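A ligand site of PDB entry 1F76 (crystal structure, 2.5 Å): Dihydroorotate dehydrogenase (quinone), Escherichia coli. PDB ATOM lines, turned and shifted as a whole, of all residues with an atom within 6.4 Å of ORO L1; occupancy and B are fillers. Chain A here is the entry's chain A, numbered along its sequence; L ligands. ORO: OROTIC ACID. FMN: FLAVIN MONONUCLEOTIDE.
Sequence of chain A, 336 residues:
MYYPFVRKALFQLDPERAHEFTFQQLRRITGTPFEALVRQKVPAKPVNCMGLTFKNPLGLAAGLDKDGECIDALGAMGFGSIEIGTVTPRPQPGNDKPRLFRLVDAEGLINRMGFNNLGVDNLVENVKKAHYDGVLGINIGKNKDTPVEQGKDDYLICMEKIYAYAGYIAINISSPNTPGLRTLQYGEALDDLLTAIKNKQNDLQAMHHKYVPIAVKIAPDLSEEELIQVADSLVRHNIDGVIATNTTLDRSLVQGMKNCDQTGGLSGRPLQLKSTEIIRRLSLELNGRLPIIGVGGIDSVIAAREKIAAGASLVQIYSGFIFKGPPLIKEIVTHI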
ATOM      1  N   LYS A  66     -30.178  -8.993 -20.575  1.00  0.00           N
ATOM      2  CA  LYS A  66     -29.295  -9.630 -19.605  1.00  0.00           C
ATOM      3  C   LYS A  66     -29.604  -9.327 -18.144  1.00  0.00           C
ATOM      4  O   LYS A  66     -29.462 -10.195 -17.291  1.00  0.00           O
ATOM      5  CB  LYS A  66     -27.837  -9.274 -19.943  1.00  0.00           C
ATOM      6  CG  LYS A  66     -27.330  -9.996 -21.192  1.00  0.00           C
ATOM      7  CD  LYS A  66     -26.147  -9.310 -21.856  1.00  0.00           C
ATOM      8  CE  LYS A  66     -24.862 -10.144 -21.768  1.00  0.00           C
ATOM      9  NZ  LYS A  66     -24.954 -11.513 -22.380  1.00  0.00           N
ATOM     10  N   THR A  86     -27.656 -13.997 -19.521  1.00  0.00           N
ATOM     11  CA  THR A  86     -27.024 -14.633 -18.371  1.00  0.00           C
ATOM     12  C   THR A  86     -26.588 -13.674 -17.259  1.00  0.00           C
ATOM     13  O   THR A  86     -25.974 -12.639 -17.515  1.00  0.00           O
ATOM     14  CB  THR A  86     -25.775 -15.428 -18.812  1.00  0.00           C
ATOM     15  OG1 THR A  86     -26.169 -16.541 -19.620  1.00  0.00           O
ATOM     16  CG2 THR A  86     -24.997 -15.933 -17.613  1.00  0.00           C
ATOM     17  N   ASN A  95     -15.968  -8.580 -21.848  1.00  0.00           N
ATOM     18  CA  ASN A  95     -14.760  -8.353 -22.634  1.00  0.00           C
ATOM     19  C   ASN A  95     -14.651  -6.946 -23.208  1.00  0.00           C
ATOM     20  O   ASN A  95     -15.610  -6.161 -23.174  1.00  0.00           O
ATOM     21  CB  ASN A  95     -14.682  -9.394 -23.758  1.00  0.00           C
ATOM     22  CG  ASN A  95     -14.689 -10.821 -23.232  1.00  0.00           C
ATOM     23  OD1 ASN A  95     -14.006 -11.138 -22.261  1.00  0.00           O
ATOM     24  ND2 ASN A  95     -15.453 -11.698 -23.873  1.00  0.00           N
ATOM     25  N   ASN A 111     -20.493 -12.556 -31.547  1.00  0.00           N
ATOM     26  CA  ASN A 111     -20.312 -11.818 -30.311  1.00  0.00           C
ATOM     27  C   ASN A 111     -19.359 -12.520 -29.356  1.00  0.00           C
ATOM     28  O   ASN A 111     -19.181 -13.751 -29.413  1.00  0.00           O
ATOM     29  CB  ASN A 111     -21.649 -11.605 -29.593  1.00  0.00           C
ATOM     30  CG  ASN A 111     -21.991 -12.754 -28.656  1.00  0.00           C
ATOM     31  OD1 ASN A 111     -21.455 -12.699 -27.438  1.00  0.00           O
ATOM     32  ND2 ASN A 111     -22.712 -13.685 -29.021  1.00  0.00           N
ATOM     33  N   ARG A 112     -18.749 -11.734 -28.491  1.00  0.00           N
ATOM     34  CA  ARG A 112     -17.844 -12.204 -27.455  1.00  0.00           C
ATOM     35  C   ARG A 112     -18.044 -11.252 -26.284  1.00  0.00           C
ATOM     36  O   ARG A 112     -17.086 -10.707 -25.734  1.00  0.00           O
ATOM     37  CB  ARG A 112     -16.379 -12.192 -27.948  1.00  0.00           C
ATOM     38  CG  ARG A 112     -15.857 -10.889 -28.522  1.00  0.00           C
ATOM     39  CD  ARG A 112     -14.367 -11.002 -28.794  1.00  0.00           C
ATOM     40  NE  ARG A 112     -13.767  -9.820 -29.415  1.00  0.00           N
ATOM     41  CZ  ARG A 112     -13.568  -9.676 -30.720  1.00  0.00           C
ATOM     42  NH1 ARG A 112     -13.020  -8.565 -31.195  1.00  0.00           N
ATOM     43  NH2 ARG A 112     -13.910 -10.635 -31.560  1.00  0.00           N
ATOM     44  N   MET A 113     -19.312 -11.064 -25.912  1.00  0.00           N
ATOM     45  CA  MET A 113     -19.702 -10.183 -24.814  1.00  0.00           C
ATOM     46  C   MET A 113     -18.965 -10.512 -23.513  1.00  0.00           C
ATOM     47  O   MET A 113     -18.402  -9.623 -22.871  1.00  0.00           O
ATOM     48  CB  MET A 113     -21.213 -10.280 -24.569  1.00  0.00           C
ATOM     49  CG  MET A 113     -22.086 -10.056 -25.805  1.00  0.00           C
ATOM     50  SD  MET A 113     -21.909  -8.298 -26.604  1.00  0.00           S
ATOM     51  CE  MET A 113     -23.033  -7.307 -25.397  1.00  0.00           C
ATOM     52  N   GLY A 114     -18.993 -11.779 -23.121  1.00  0.00           N
ATOM     53  CA  GLY A 114     -18.337 -12.210 -21.904  1.00  0.00           C
ATOM     54  C   GLY A 114     -19.154 -12.023 -20.641  1.00  0.00           C
ATOM     55  O   GLY A 114     -18.624 -11.629 -19.606  1.00  0.00           O
ATOM     56  N   PHE A 115     -20.451 -12.301 -20.706  1.00  0.00           N
ATOM     57  CA  PHE A 115     -21.345 -12.163 -19.563  1.00  0.00           C
ATOM     58  C   PHE A 115     -21.346 -10.771 -18.925  1.00  0.00           C
ATOM     59  O   PHE A 115     -21.192 -10.645 -17.704  1.00  0.00           O
ATOM     60  CB  PHE A 115     -21.018 -13.199 -18.471  1.00  0.00           C
ATOM     61  CG  PHE A 115     -21.367 -14.615 -18.834  1.00  0.00           C
ATOM     62  CD1 PHE A 115     -22.284 -14.888 -19.846  1.00  0.00           C
ATOM     63  CD2 PHE A 115     -20.797 -15.681 -18.135  1.00  0.00           C
ATOM     64  CE1 PHE A 115     -22.640 -16.211 -20.153  1.00  0.00           C
ATOM     65  CE2 PHE A 115     -21.144 -16.997 -18.419  1.00  0.00           C
ATOM     66  CZ  PHE A 115     -22.072 -17.272 -19.441  1.00  0.00           C
ATOM     67  N   ASN A 116     -21.511  -9.737 -19.737  1.00  0.00           N
ATOM     68  CA  ASN A 116     -21.559  -8.384 -19.178  1.00  0.00           C
ATOM     69  C   ASN A 116     -22.911  -8.227 -18.487  1.00  0.00           C
ATOM     70  O   ASN A 116     -23.958  -8.262 -19.132  1.00  0.00           O
ATOM     71  CB  ASN A 116     -21.414  -7.335 -20.295  1.00  0.00           C
ATOM     72  CG  ASN A 116     -22.448  -7.502 -21.409  1.00  0.00           C
ATOM     73  OD1 ASN A 116     -22.511  -8.551 -22.066  1.00  0.00           O
ATOM     74  ND2 ASN A 116     -23.258  -6.473 -21.620  1.00  0.00           N
ATOM     75  N   ASN A 139     -31.582 -17.243 -16.631  1.00  0.00           N
ATOM     76  CA  ASN A 139     -30.366 -17.876 -17.117  1.00  0.00           C
ATOM     77  C   ASN A 139     -29.171 -17.404 -16.284  1.00  0.00           C
ATOM     78  O   ASN A 139     -28.918 -16.207 -16.174  1.00  0.00           O
ATOM     79  CB  ASN A 139     -30.197 -17.534 -18.594  1.00  0.00           C
ATOM     80  CG  ASN A 139     -29.032 -18.220 -19.239  1.00  0.00           C
ATOM     81  OD1 ASN A 139     -27.891 -18.068 -18.820  1.00  0.00           O
ATOM     82  ND2 ASN A 139     -29.318 -18.993 -20.283  1.00  0.00           N
ATOM     83  N   ASN A 172     -26.313 -22.006 -17.786  1.00  0.00           N
ATOM     84  CA  ASN A 172     -25.467 -21.748 -18.942  1.00  0.00           C
ATOM     85  C   ASN A 172     -24.044 -22.274 -18.795  1.00  0.00           C
ATOM     86  O   ASN A 172     -23.211 -21.688 -18.109  1.00  0.00           O
ATOM     87  CB  ASN A 172     -25.424 -20.239 -19.252  1.00  0.00           C
ATOM     88  CG  ASN A 172     -24.629 -19.932 -20.521  1.00  0.00           C
ATOM     89  OD1 ASN A 172     -24.038 -20.821 -21.145  1.00  0.00           O
ATOM     90  ND2 ASN A 172     -24.603 -18.660 -20.900  1.00  0.00           N
ATOM     91  N   SER A 174     -22.544 -23.279 -21.797  1.00  0.00           N
ATOM     92  CA  SER A 174     -22.216 -23.368 -23.219  1.00  0.00           C
ATOM     93  C   SER A 174     -21.665 -22.119 -23.883  1.00  0.00           C
ATOM     94  O   SER A 174     -21.327 -22.143 -25.058  1.00  0.00           O
ATOM     95  CB  SER A 174     -23.430 -23.887 -24.000  1.00  0.00           C
ATOM     96  OG  SER A 174     -24.602 -23.171 -23.667  1.00  0.00           O
ATOM     97  N   SER A 175     -21.559 -21.023 -23.143  1.00  0.00           N
ATOM     98  CA  SER A 175     -21.022 -19.788 -23.712  1.00  0.00           C
ATOM     99  C   SER A 175     -19.582 -19.998 -24.126  1.00  0.00           C
ATOM    100  O   SER A 175     -18.795 -20.609 -23.408  1.00  0.00           O
ATOM    101  CB  SER A 175     -21.062 -18.654 -22.692  1.00  0.00           C
ATOM    102  OG  SER A 175     -20.305 -17.547 -23.177  1.00  0.00           O
ATOM    103  N   PRO A 176     -19.212 -19.482 -25.313  1.00  0.00           N
ATOM    104  CA  PRO A 176     -17.831 -19.646 -25.764  1.00  0.00           C
ATOM    105  C   PRO A 176     -16.965 -18.440 -25.395  1.00  0.00           C
ATOM    106  O   PRO A 176     -15.778 -18.400 -25.693  1.00  0.00           O
ATOM    107  CB  PRO A 176     -17.986 -19.774 -27.277  1.00  0.00           C
ATOM    108  CG  PRO A 176     -19.076 -18.777 -27.540  1.00  0.00           C
ATOM    109  CD  PRO A 176     -20.082 -19.056 -26.424  1.00  0.00           C
ATOM    110  N   ASN A 177     -17.570 -17.465 -24.707  1.00  0.00           N
ATOM    111  CA  ASN A 177     -16.845 -16.252 -24.361  1.00  0.00           C
ATOM    112  C   ASN A 177     -16.283 -16.139 -22.946  1.00  0.00           C
ATOM    113  O   ASN A 177     -15.801 -15.086 -22.543  1.00  0.00           O
ATOM    114  CB  ASN A 177     -17.720 -15.045 -24.691  1.00  0.00           C
ATOM    115  CG  ASN A 177     -18.231 -15.085 -26.124  1.00  0.00           C
ATOM    116  OD1 ASN A 177     -17.480 -15.336 -27.062  1.00  0.00           O
ATOM    117  ND2 ASN A 177     -19.526 -14.854 -26.303  1.00  0.00           N
ATOM    118  N   THR A 178     -16.334 -17.237 -22.199  1.00  0.00           N
ATOM    119  CA  THR A 178     -15.786 -17.286 -20.848  1.00  0.00           C
ATOM    120  C   THR A 178     -14.838 -18.482 -20.831  1.00  0.00           C
ATOM    121  O   THR A 178     -15.267 -19.630 -20.964  1.00  0.00           O
ATOM    122  CB  THR A 178     -16.885 -17.458 -19.784  1.00  0.00           C
ATOM    123  OG1 THR A 178     -17.739 -16.307 -19.803  1.00  0.00           O
ATOM    124  CG2 THR A 178     -16.262 -17.579 -18.398  1.00  0.00           C
ATOM    125  N   LEU A 181     -15.493 -22.328 -19.676  1.00  0.00           N
ATOM    126  CA  LEU A 181     -16.897 -22.576 -19.375  1.00  0.00           C
ATOM    127  C   LEU A 181     -17.517 -23.795 -20.035  1.00  0.00           C
ATOM    128  O   LEU A 181     -18.359 -24.458 -19.442  1.00  0.00           O
ATOM    129  CB  LEU A 181     -17.746 -21.355 -19.727  1.00  0.00           C
ATOM    130  CG  LEU A 181     -19.146 -21.463 -19.109  1.00  0.00           C
ATOM    131  CD1 LEU A 181     -19.013 -21.255 -17.607  1.00  0.00           C
ATOM    132  CD2 LEU A 181     -20.092 -20.420 -19.698  1.00  0.00           C
ATOM    133  N   LYS A 217     -28.388 -25.452 -20.834  1.00  0.00           N
ATOM    134  CA  LYS A 217     -28.131 -24.958 -22.189  1.00  0.00           C
ATOM    135  C   LYS A 217     -26.792 -25.421 -22.736  1.00  0.00           C
ATOM    136  O   LYS A 217     -25.731 -25.020 -22.257  1.00  0.00           O
ATOM    137  CB  LYS A 217     -28.200 -23.428 -22.200  1.00  0.00           C
ATOM    138  CG  LYS A 217     -28.201 -22.820 -23.604  1.00  0.00           C
ATOM    139  CD  LYS A 217     -28.591 -21.351 -23.572  1.00  0.00           C
ATOM    140  CE  LYS A 217     -28.619 -20.736 -24.968  1.00  0.00           C
ATOM    141  NZ  LYS A 217     -29.010 -19.305 -24.907  1.00  0.00           N
ATOM    142  N   ASN A 246     -26.652 -23.061 -28.180  1.00  0.00           N
ATOM    143  CA  ASN A 246     -25.983 -21.769 -27.968  1.00  0.00           C
ATOM    144  C   ASN A 246     -25.283 -21.394 -29.281  1.00  0.00           C
ATOM    145  O   ASN A 246     -25.473 -22.051 -30.303  1.00  0.00           O
ATOM    146  CB  ASN A 246     -24.951 -21.868 -26.839  1.00  0.00           C
ATOM    147  CG  ASN A 246     -24.717 -20.528 -26.125  1.00  0.00           C
ATOM    148  OD1 ASN A 246     -24.427 -19.509 -26.764  1.00  0.00           O
ATOM    149  ND2 ASN A 246     -24.831 -20.536 -24.801  1.00  0.00           N
ATOM    150  N   THR A 247     -24.446 -20.365 -29.259  1.00  0.00           N
ATOM    151  CA  THR A 247     -23.747 -19.947 -30.481  1.00  0.00           C
ATOM    152  C   THR A 247     -22.586 -20.872 -30.853  1.00  0.00           C
ATOM    153  O   THR A 247     -22.035 -21.571 -30.011  1.00  0.00           O
ATOM    154  CB  THR A 247     -23.231 -18.524 -30.333  1.00  0.00           C
ATOM    155  OG1 THR A 247     -22.247 -18.474 -29.293  1.00  0.00           O
ATOM    156  CG2 THR A 247     -24.386 -17.609 -29.987  1.00  0.00           C
ATOM    157  N   GLY A 264     -15.415 -15.267 -31.373  1.00  0.00           N
ATOM    158  CA  GLY A 264     -16.695 -15.219 -30.681  1.00  0.00           C
ATOM    159  C   GLY A 264     -17.674 -16.284 -31.118  1.00  0.00           C
ATOM    160  O   GLY A 264     -17.310 -17.197 -31.856  1.00  0.00           O
ATOM    161  N   GLY A 265     -18.916 -16.162 -30.677  1.00  0.00           N
ATOM    162  CA  GLY A 265     -19.932 -17.119 -31.069  1.00  0.00           C
ATOM    163  C   GLY A 265     -20.790 -16.591 -32.201  1.00  0.00           C
ATOM    164  O   GLY A 265     -21.226 -15.432 -32.193  1.00  0.00           O
ATOM    165  N   LEU A 266     -21.035 -17.439 -33.194  1.00  0.00           N
ATOM    166  CA  LEU A 266     -21.833 -17.081 -34.365  1.00  0.00           C
ATOM    167  C   LEU A 266     -23.290 -17.502 -34.179  1.00  0.00           C
ATOM    168  O   LEU A 266     -23.571 -18.624 -33.761  1.00  0.00           O
ATOM    169  CB  LEU A 266     -21.247 -17.760 -35.614  1.00  0.00           C
ATOM    170  CG  LEU A 266     -21.939 -17.637 -36.975  1.00  0.00           C
ATOM    171  CD1 LEU A 266     -21.909 -16.189 -37.466  1.00  0.00           C
ATOM    172  CD2 LEU A 266     -21.219 -18.535 -37.961  1.00  0.00           C
ATOM    173  N   SER A 267     -24.214 -16.601 -34.488  1.00  0.00           N
ATOM    174  CA  SER A 267     -25.636 -16.879 -34.356  1.00  0.00           C
ATOM    175  C   SER A 267     -26.385 -16.466 -35.615  1.00  0.00           C
ATOM    176  O   SER A 267     -25.772 -15.973 -36.567  1.00  0.00           O
ATOM    177  CB  SER A 267     -26.215 -16.110 -33.163  1.00  0.00           C
ATOM    178  OG  SER A 267     -25.981 -14.717 -33.314  1.00  0.00           O
HETATM  179  N1  ORO L   1     -22.280 -14.994 -25.846  1.00  0.00           N
HETATM  180  C2  ORO L   1     -22.846 -16.084 -26.536  1.00  0.00           C
HETATM  181  O2  ORO L   1     -22.851 -16.170 -27.773  1.00  0.00           O
HETATM  182  N3  ORO L   1     -23.387 -17.061 -25.703  1.00  0.00           N
HETATM  183  C4  ORO L   1     -23.430 -17.052 -24.301  1.00  0.00           C
HETATM  184  O4  ORO L   1     -23.938 -17.967 -23.669  1.00  0.00           O
HETATM  185  C5  ORO L   1     -22.827 -15.884 -23.656  1.00  0.00           C
HETATM  186  C6  ORO L   1     -22.288 -14.905 -24.444  1.00  0.00           C
HETATM  187  C7  ORO L   1     -21.635 -13.662 -23.848  1.00  0.00           C
HETATM  188  O71 ORO L   1     -22.332 -12.974 -23.048  1.00  0.00           O
HETATM  189  O72 ORO L   1     -20.462 -13.452 -24.212  1.00  0.00           O
HETATM  190  N1  FMN L   2     -27.053 -17.095 -24.479  1.00  0.00           N
HETATM  191  C2  FMN L   2     -27.079 -17.304 -23.091  1.00  0.00           C
HETATM  192  O2  FMN L   2     -27.443 -18.377 -22.694  1.00  0.00           O
HETATM  193  N3  FMN L   2     -26.669 -16.220 -22.254  1.00  0.00           N
HETATM  194  C4  FMN L   2     -26.249 -14.981 -22.787  1.00  0.00           C
HETATM  195  O4  FMN L   2     -25.882 -14.067 -22.034  1.00  0.00           O
HETATM  196  C4A FMN L   2     -26.225 -14.893 -24.260  1.00  0.00           C
HETATM  197  N5  FMN L   2     -25.831 -13.585 -24.786  1.00  0.00           N
HETATM  198  C5A FMN L   2     -26.018 -13.362 -26.029  1.00  0.00           C
HETATM  199  C6  FMN L   2     -25.722 -12.085 -26.578  1.00  0.00           C
HETATM  200  C7  FMN L   2     -25.707 -11.877 -27.975  1.00  0.00           C
HETATM  201  C7M FMN L   2     -25.322 -10.493 -28.623  1.00  0.00           C
HETATM  202  C8  FMN L   2     -26.006 -12.957 -28.876  1.00  0.00           C
HETATM  203  C8M FMN L   2     -26.006 -12.827 -30.415  1.00  0.00           C
HETATM  204  C9  FMN L   2     -26.303 -14.233 -28.358  1.00  0.00           C
HETATM  205  C9A FMN L   2     -26.330 -14.460 -26.987  1.00  0.00           C
HETATM  206  N10 FMN L   2     -26.669 -15.805 -26.529  1.00  0.00           N
HETATM  207  C10 FMN L   2     -26.684 -15.951 -25.132  1.00  0.00           C
HETATM  208  C1' FMN L   2     -27.019 -16.854 -27.344  1.00  0.00           C
HETATM  209  C2' FMN L   2     -28.580 -16.906 -27.655  1.00  0.00           C
HETATM  210  O2' FMN L   2     -29.402 -16.938 -26.457  1.00  0.00           O
HETATM  211  C3' FMN L   2     -28.880 -18.068 -28.618  1.00  0.00           C
HETATM  212  O3' FMN L   2     -28.679 -19.229 -27.835  1.00  0.00           O
HETATM  213  C4' FMN L   2     -28.050 -18.072 -30.024  1.00  0.00           C
HETATM  214  O4' FMN L   2     -27.727 -16.719 -30.412  1.00  0.00           O
HETATM  215  C5' FMN L   2     -28.841 -18.821 -31.002  1.00  0.00           C
HETATM  216  O5' FMN L   2     -30.121 -18.227 -31.391  1.00  0.00           O
HETATM  217  P   FMN L   2     -30.273 -17.096 -32.560  1.00  0.00           P
HETATM  218  O1P FMN L   2     -31.762 -17.133 -32.816  1.00  0.00           O
HETATM  219  O2P FMN L   2     -29.629 -15.879 -32.133  1.00  0.00           O
HETATM  220  O3P FMN L   2     -29.625 -17.699 -33.817  1.00  0.00           O
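Arg 112 touches ORO L1 (C to O72, 3.9 Å).
Ser 175 touches ORO L1 (OG to C5, 3.1 Å).
Pro 176 touches ORO L1.
Hydrophobic or aromatic side chains that line ORO L1: Met 113, Phe 115 and Pro 176.
Of the 24 residues printed, 12 come within 4 Å of ORO L1.
The nearest printed residue that does not touch ORO L1 is Gly 265 (4.5 Å).
N of Gly 114 sits at hydrogen-bond distance from O72 of ORO L1 (2.5 Å).
O72 of ORO L1 is in hydrogen-bond range of ND2 of Asn 177.
An oxygen (O2) of ORO L1 sits at hydrogen-bond distance from the side-chain amide nitrogen of Asn 111.
OG1 of Thr 247 is in hydrogen-bond range of O2 of ORO L1 (2.8 Å).
N3 of ORO L1 sits at hydrogen-bond distance from OD1 of Asn 246.
ND2 of Asn 172 is in hydrogen-bond range of O4 of ORO L1 (2.9 Å).
O71 of ORO L1 lies within salt-bridge range of NZ of Lys 66, at 3.1 Å.
The backbone NH of Phe 115 sits at hydrogen-bond distance from an oxygen (O71) of ORO L1 (3.1 Å).
The backbone NH (N) of Met 113 is in hydrogen-bond range of an oxygen (O72) of ORO L1 (3.1 Å).
The side-chain amide nitrogen (ND2) of Asn 172 lies within hydrogen-bond range of an oxygen (O2) of FMN L2, 3.4 Å away.
The side-chain amino group (NZ) of Lys 66 lies within hydrogen-bond range of an oxygen (O4) of FMN L2 (2.7 Å).
O4 of FMN L2 lies within hydrogen-bond range of N of Thr 86, at 3.1 Å.
A nitrogen (N3) of FMN L2 sits at hydrogen-bond distance from the side-chain hydroxyl of Thr 86, at 2.7 Å.
NZ of Lys 217 sits at hydrogen-bond distance from O2' of FMN L2 (2.9 Å).
The side-chain amide nitrogen of Asn 139 lies within hydrogen-bond range of an oxygen (O2) of FMN L2, at 3.1 Å.
The side-chain hydroxyl (OG) of Ser 175 sits at hydrogen-bond distance from the backbone NH (N) of Asn 177 (3.1 Å).
The side-chain amide oxygen of Asn 111 sits at hydrogen-bond distance from the backbone NH of Met 113, at 3.1 Å.
O of Asn 111 sits at hydrogen-bond distance from N of Gly 265, 2.7 Å away.
The side-chain amide nitrogen (ND2) of Asn 246 lies within hydrogen-bond range of the side-chain hydroxyl (OG) of Ser 174 (2.9 Å).
The side-chain amide oxygen of Asn 172 sits at hydrogen-bond distance from the backbone NH of Ser 175 (3.2 Å).
The side-chain amide oxygen (OD1) of Asn 172 lies within hydrogen-bond range of the backbone NH (N) of Ser 174.
ND2 of Asn 172 sits at hydrogen-bond distance from OG1 of Thr 86 (2.9 Å).
The side-chain amide nitrogen (ND2) of Asn 95 sits at hydrogen-bond distance from the backbone carbonyl oxygen (O) of Arg 112 (2.7 Å).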
